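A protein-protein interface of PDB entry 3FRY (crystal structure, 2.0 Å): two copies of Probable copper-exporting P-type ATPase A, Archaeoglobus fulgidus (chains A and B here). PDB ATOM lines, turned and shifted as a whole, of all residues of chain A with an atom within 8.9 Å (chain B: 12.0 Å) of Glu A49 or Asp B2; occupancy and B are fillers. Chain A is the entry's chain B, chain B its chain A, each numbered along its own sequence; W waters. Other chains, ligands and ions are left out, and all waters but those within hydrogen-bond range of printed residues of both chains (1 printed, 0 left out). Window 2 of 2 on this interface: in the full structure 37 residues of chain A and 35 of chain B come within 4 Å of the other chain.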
ATOM      1  N   GLY A  46     -13.220  14.241 -17.296  1.00  0.00           N
ATOM      2  CA  GLY A  46     -12.963  13.054 -16.513  1.00  0.00           C
ATOM      3  C   GLY A  46     -13.614  11.805 -17.053  1.00  0.00           C
ATOM      4  O   GLY A  46     -14.028  11.750 -18.211  1.00  0.00           O
ATOM      5  N   ASN A  47     -13.704  10.798 -16.194  1.00  0.00           N
ATOM      6  CA  ASN A  47     -14.300   9.527 -16.563  1.00  0.00           C
ATOM      7  C   ASN A  47     -15.758   9.482 -16.118  1.00  0.00           C
ATOM      8  O   ASN A  47     -16.071   9.700 -14.945  1.00  0.00           O
ATOM      9  CB  ASN A  47     -13.505   8.395 -15.921  1.00  0.00           C
ATOM     10  CG  ASN A  47     -12.016   8.523 -16.181  1.00  0.00           C
ATOM     11  OD1 ASN A  47     -11.575   8.562 -17.333  1.00  0.00           O
ATOM     12  ND2 ASN A  47     -11.234   8.598 -15.113  1.00  0.00           N
ATOM     13  N   LYS A  48     -16.644   9.203 -17.069  1.00  0.00           N
ATOM     14  CA  LYS A  48     -18.071   9.138 -16.797  1.00  0.00           C
ATOM     15  C   LYS A  48     -18.373   8.197 -15.635  1.00  0.00           C
ATOM     16  O   LYS A  48     -19.329   8.414 -14.885  1.00  0.00           O
ATOM     17  CB  LYS A  48     -18.823   8.687 -18.057  1.00  0.00           C
ATOM     18  CG  LYS A  48     -20.343   8.779 -17.953  1.00  0.00           C
ATOM     19  CD  LYS A  48     -21.017   8.614 -19.316  1.00  0.00           C
ATOM     20  CE  LYS A  48     -20.904   7.193 -19.851  1.00  0.00           C
ATOM     21  NZ  LYS A  48     -21.725   6.228 -19.062  1.00  0.00           N
ATOM     22  N   GLU A  49     -17.553   7.162 -15.476  1.00  0.00           N
ATOM     23  CA  GLU A  49     -17.760   6.202 -14.398  1.00  0.00           C
ATOM     24  C   GLU A  49     -17.316   6.726 -13.035  1.00  0.00           C
ATOM     25  O   GLU A  49     -17.652   6.140 -12.007  1.00  0.00           O
ATOM     26  CB  GLU A  49     -17.042   4.876 -14.698  1.00  0.00           C
ATOM     27  CG  GLU A  49     -15.525   4.897 -14.557  1.00  0.00           C
ATOM     28  CD  GLU A  49     -14.821   5.562 -15.725  1.00  0.00           C
ATOM     29  OE1 GLU A  49     -13.573   5.500 -15.769  1.00  0.00           O
ATOM     30  OE2 GLU A  49     -15.504   6.145 -16.596  1.00  0.00           O
ATOM     31  N   ASP A  50     -16.564   7.824 -13.025  1.00  0.00           N
ATOM     32  CA  ASP A  50     -16.097   8.411 -11.769  1.00  0.00           C
ATOM     33  C   ASP A  50     -16.978   9.567 -11.296  1.00  0.00           C
ATOM     34  O   ASP A  50     -16.620  10.281 -10.359  1.00  0.00           O
ATOM     35  CB  ASP A  50     -14.655   8.907 -11.903  1.00  0.00           C
ATOM     36  CG  ASP A  50     -13.647   7.776 -11.945  1.00  0.00           C
ATOM     37  OD1 ASP A  50     -13.921   6.713 -11.348  1.00  0.00           O
ATOM     38  OD2 ASP A  50     -12.573   7.955 -12.561  1.00  0.00           O
ATOM     39  N   VAL A  51     -18.125   9.747 -11.944  1.00  0.00           N
ATOM     40  CA  VAL A  51     -19.045  10.818 -11.578  1.00  0.00           C
ATOM     41  C   VAL A  51     -19.399  10.791 -10.094  1.00  0.00           C
ATOM     42  O   VAL A  51     -19.205  11.782  -9.386  1.00  0.00           O
ATOM     43  CB  VAL A  51     -20.336  10.750 -12.428  1.00  0.00           C
ATOM     44  CG1 VAL A  51     -21.444  11.584 -11.794  1.00  0.00           C
ATOM     45  CG2 VAL A  51     -20.045  11.267 -13.829  1.00  0.00           C
ATOM     46  N   ASP A  52     -19.906   9.660  -9.616  1.00  0.00           N
ATOM     47  CA  ASP A  52     -20.270   9.552  -8.206  1.00  0.00           C
ATOM     48  C   ASP A  52     -19.053   9.838  -7.321  1.00  0.00           C
ATOM     49  O   ASP A  52     -19.173  10.444  -6.258  1.00  0.00           O
ATOM     50  CB  ASP A  52     -20.833   8.161  -7.907  1.00  0.00           C
ATOM     51  CG  ASP A  52     -21.389   8.052  -6.505  1.00  0.00           C
ATOM     52  OD1 ASP A  52     -20.589   8.048  -5.542  1.00  0.00           O
ATOM     53  OD2 ASP A  52     -22.628   7.978  -6.363  1.00  0.00           O
ATOM     54  N   LYS A  53     -17.885   9.403  -7.779  1.00  0.00           N
ATOM     55  CA  LYS A  53     -16.633   9.618  -7.058  1.00  0.00           C
ATOM     56  C   LYS A  53     -16.344  11.110  -6.924  1.00  0.00           C
ATOM     57  O   LYS A  53     -15.947  11.584  -5.858  1.00  0.00           O
ATOM     58  CB  LYS A  53     -15.493   8.929  -7.809  1.00  0.00           C
ATOM     59  CG  LYS A  53     -14.083   9.219  -7.308  1.00  0.00           C
ATOM     60  CD  LYS A  53     -13.082   8.351  -8.078  1.00  0.00           C
ATOM     61  CE  LYS A  53     -11.633   8.732  -7.810  1.00  0.00           C
ATOM     62  NZ  LYS A  53     -11.274   8.607  -6.379  1.00  0.00           N
ATOM     63  N   TYR A  54     -16.540  11.855  -8.006  1.00  0.00           N
ATOM     64  CA  TYR A  54     -16.293  13.292  -7.970  1.00  0.00           C
ATOM     65  C   TYR A  54     -17.300  13.975  -7.046  1.00  0.00           C
ATOM     66  O   TYR A  54     -16.949  14.883  -6.298  1.00  0.00           O
ATOM     67  CB  TYR A  54     -16.390  13.902  -9.373  1.00  0.00           C
ATOM     68  CG  TYR A  54     -15.489  13.267 -10.415  1.00  0.00           C
ATOM     69  CD1 TYR A  54     -14.216  12.804 -10.085  1.00  0.00           C
ATOM     70  CD2 TYR A  54     -15.901  13.166 -11.747  1.00  0.00           C
ATOM     71  CE1 TYR A  54     -13.376  12.256 -11.055  1.00  0.00           C
ATOM     72  CE2 TYR A  54     -15.071  12.623 -12.719  1.00  0.00           C
ATOM     73  CZ  TYR A  54     -13.812  12.169 -12.369  1.00  0.00           C
ATOM     74  OH  TYR A  54     -12.997  11.620 -13.333  1.00  0.00           O
ATOM     75  N   GLY B   1      -6.161   3.445 -20.522  1.00  0.00           N
ATOM     76  CA  GLY B   1      -6.894   3.671 -21.734  1.00  0.00           C
ATOM     77  C   GLY B   1      -8.483   3.931 -21.730  1.00  0.00           C
ATOM     78  O   GLY B   1      -9.149   3.779 -22.711  1.00  0.00           O
ATOM     79  N   ASP B   2      -8.988   4.385 -20.550  1.00  0.00           N
ATOM     80  CA  ASP B   2     -10.384   4.711 -20.324  1.00  0.00           C
ATOM     81  C   ASP B   2     -10.755   5.922 -21.189  1.00  0.00           C
ATOM     82  O   ASP B   2      -9.906   6.385 -21.803  1.00  0.00           O
ATOM     83  CB  ASP B   2     -10.657   4.986 -18.824  1.00  0.00           C
ATOM     84  CG  ASP B   2     -10.712   3.694 -17.942  1.00  0.00           C
ATOM     85  OD1 ASP B   2     -11.186   2.747 -18.396  1.00  0.00           O
ATOM     86  OD2 ASP B   2     -10.259   3.625 -16.810  1.00  0.00           O
ATOM     87  N   SER B   3     -11.972   6.391 -21.182  1.00  0.00           N
ATOM     88  CA  SER B   3     -12.330   7.496 -21.942  1.00  0.00           C
ATOM     89  C   SER B   3     -12.702   8.853 -21.271  1.00  0.00           C
ATOM     90  O   SER B   3     -13.370   8.807 -20.415  1.00  0.00           O
ATOM     91  CB  SER B   3     -13.396   6.937 -22.782  1.00  0.00           C
ATOM     92  OG  SER B   3     -13.943   7.879 -23.492  1.00  0.00           O
ATOM     93  N   VAL B   4     -12.099  10.084 -21.732  1.00  0.00           N
ATOM     94  CA  VAL B   4     -12.266  11.392 -21.100  1.00  0.00           C
ATOM     95  C   VAL B   4     -13.422  12.146 -21.721  1.00  0.00           C
ATOM     96  O   VAL B   4     -13.407  12.366 -22.908  1.00  0.00           O
ATOM     97  CB  VAL B   4     -10.993  12.279 -21.235  1.00  0.00           C
ATOM     98  CG1 VAL B   4     -11.173  13.438 -20.677  1.00  0.00           C
ATOM     99  CG2 VAL B   4      -9.944  11.587 -20.684  1.00  0.00           C
ATOM    100  N   GLU B   5     -14.335  12.633 -20.881  1.00  0.00           N
ATOM    101  CA  GLU B   5     -15.453  13.433 -21.377  1.00  0.00           C
ATOM    102  C   GLU B   5     -15.725  14.624 -20.476  1.00  0.00           C
ATOM    103  O   GLU B   5     -15.277  14.668 -19.328  1.00  0.00           O
ATOM    104  CB  GLU B   5     -16.728  12.593 -21.459  1.00  0.00           C
ATOM    105  CG  GLU B   5     -16.627  11.369 -22.343  1.00  0.00           C
ATOM    106  CD  GLU B   5     -17.989  10.789 -22.671  1.00  0.00           C
ATOM    107  OE1 GLU B   5     -18.654  11.312 -23.596  1.00  0.00           O
ATOM    108  OE2 GLU B   5     -18.401   9.821 -21.994  1.00  0.00           O
ATOM    109  N   LYS B   6     -16.467  15.592 -21.004  1.00  0.00           N
ATOM    110  CA  LYS B   6     -16.814  16.772 -20.234  1.00  0.00           C
ATOM    111  C   LYS B   6     -17.966  16.397 -19.310  1.00  0.00           C
ATOM    112  O   LYS B   6     -19.013  15.915 -19.756  1.00  0.00           O
ATOM    113  CB  LYS B   6     -17.235  17.921 -21.153  1.00  0.00           C
ATOM    114  CG  LYS B   6     -17.663  19.173 -20.394  1.00  0.00           C
ATOM    115  CD  LYS B   6     -18.141  20.273 -21.326  1.00  0.00           C
ATOM    116  CE  LYS B   6     -17.007  20.804 -22.187  1.00  0.00           C
ATOM    117  NZ  LYS B   6     -17.458  21.898 -23.099  1.00  0.00           N
ATOM    118  N   ILE B   7     -17.750  16.612 -18.019  1.00  0.00           N
ATOM    119  CA  ILE B   7     -18.735  16.303 -16.994  1.00  0.00           C
ATOM    120  C   ILE B   7     -19.069  17.597 -16.255  1.00  0.00           C
ATOM    121  O   ILE B   7     -18.170  18.295 -15.789  1.00  0.00           O
ATOM    122  CB  ILE B   7     -18.162  15.261 -15.995  1.00  0.00           C
ATOM    123  CG1 ILE B   7     -17.936  13.928 -16.721  1.00  0.00           C
ATOM    124  CG2 ILE B   7     -19.107  15.084 -14.808  1.00  0.00           C
ATOM    125  CD1 ILE B   7     -17.129  12.919 -15.924  1.00  0.00           C
ATOM    126  N   VAL B   8     -20.357  17.913 -16.156  1.00  0.00           N
ATOM    127  CA  VAL B   8     -20.790  19.136 -15.482  1.00  0.00           C
ATOM    128  C   VAL B   8     -21.547  18.834 -14.196  1.00  0.00           C
ATOM    129  O   VAL B   8     -22.517  18.070 -14.197  1.00  0.00           O
ATOM    130  CB  VAL B   8     -21.707  19.990 -16.396  1.00  0.00           C
ATOM    131  CG1 VAL B   8     -22.135  21.265 -15.671  1.00  0.00           C
ATOM    132  CG2 VAL B   8     -20.978  20.334 -17.685  1.00  0.00           C
ATOM    133  N   LEU B   9     -21.097  19.435 -13.099  1.00  0.00           N
ATOM    134  CA  LEU B   9     -21.744  19.232 -11.808  1.00  0.00           C
ATOM    135  C   LEU B   9     -22.296  20.556 -11.294  1.00  0.00           C
ATOM    136  O   LEU B   9     -21.597  21.565 -11.301  1.00  0.00           O
ATOM    137  CB  LEU B   9     -20.746  18.702 -10.775  1.00  0.00           C
ATOM    138  CG  LEU B   9     -19.868  17.484 -11.059  1.00  0.00           C
ATOM    139  CD1 LEU B   9     -19.000  17.226  -9.837  1.00  0.00           C
ATOM    140  CD2 LEU B   9     -20.723  16.261 -11.377  1.00  0.00           C
HETATM  141  O   HOH W   1     -15.715   8.529 -19.501  1.00  0.00           O
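The side-chain carboxylate of Asp A50 lies within hydrogen-bond range of the side-chain amide nitrogen of Asn A47, 3.0 Å away. N of Asn A47 is in hydrogen-bond range of OH of Tyr A54, at 3.1 Å.
Among the printed residues, pairs that only touch across the chains: Gly A46 with Val B4, Asn A47 with Ile B7, Asn A47 with Ser B3, Gly A46 with Ser B3, Tyr A54 with Ile B7, Gly A46 with Ile B7, Lys A48 with Ile B7, Lys A48 with Glu B5, Glu A49 with Asp B2, Val A51 with Ile B7 and Asn A47 with Asp B2.
Hydrophobic or aromatic side chains of chain A within 4 Å of the printed part of chain B: Val A51 and Tyr A54. Of the 9 printed residues of chain B, 5 touch a printed residue of chain A. Among the printed residues, 12 pairs touch across the chains. Among the printed residues, no Asp or Glu carboxylate lies within 4 Å of a Lys or Arg side-chain nitrogen of the other chain.
Of the printed residues of chain B, Gly A46 touches Ser B3, Val B4, Glu B5 and Ile B7. Of the printed residues of chain B, Glu A49 touches Asp B2. Val A51 touches just one residue of chain B: Ile B7 (3.95 Å). No residue of chain B comes within 4 Å of Asp A52. Lys A53 touches none of the printed residues of chain B. No residue of chain A comes within 4 Å of Gly B1. Printed residues of chain A within 4 Å of Asp B2: Asn A47 and Glu A49. Ser B3 touches two residues of chain A. Printed residues of chain A within 4 Å of Glu B5: Gly A46 and Lys A48. Leu B9 touches none of the printed residues of chain A. The nearest residue of chain B that does not touch Glu A49 is Ser B3 (5.1 Å). The nearest printed residue of chain A that does not touch Asp B2 is Asp A50 (6.5 Å). The nearest printed residue of chain A that does not touch Ile B7 is Asp A50 (5.7 Å).
No position is printed for both chains.
Water W1 lies within hydrogen-bond range of the backbone carbonyl oxygen (O) of Ser B3 (2.5 Å) and the backbone NH (N) of Lys A48 (2.7 Å).
The backbone NH (N) of Glu B5 sits at hydrogen-bond distance from the backbone carbonyl oxygen (O) of Gly A46 (2.8 Å).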
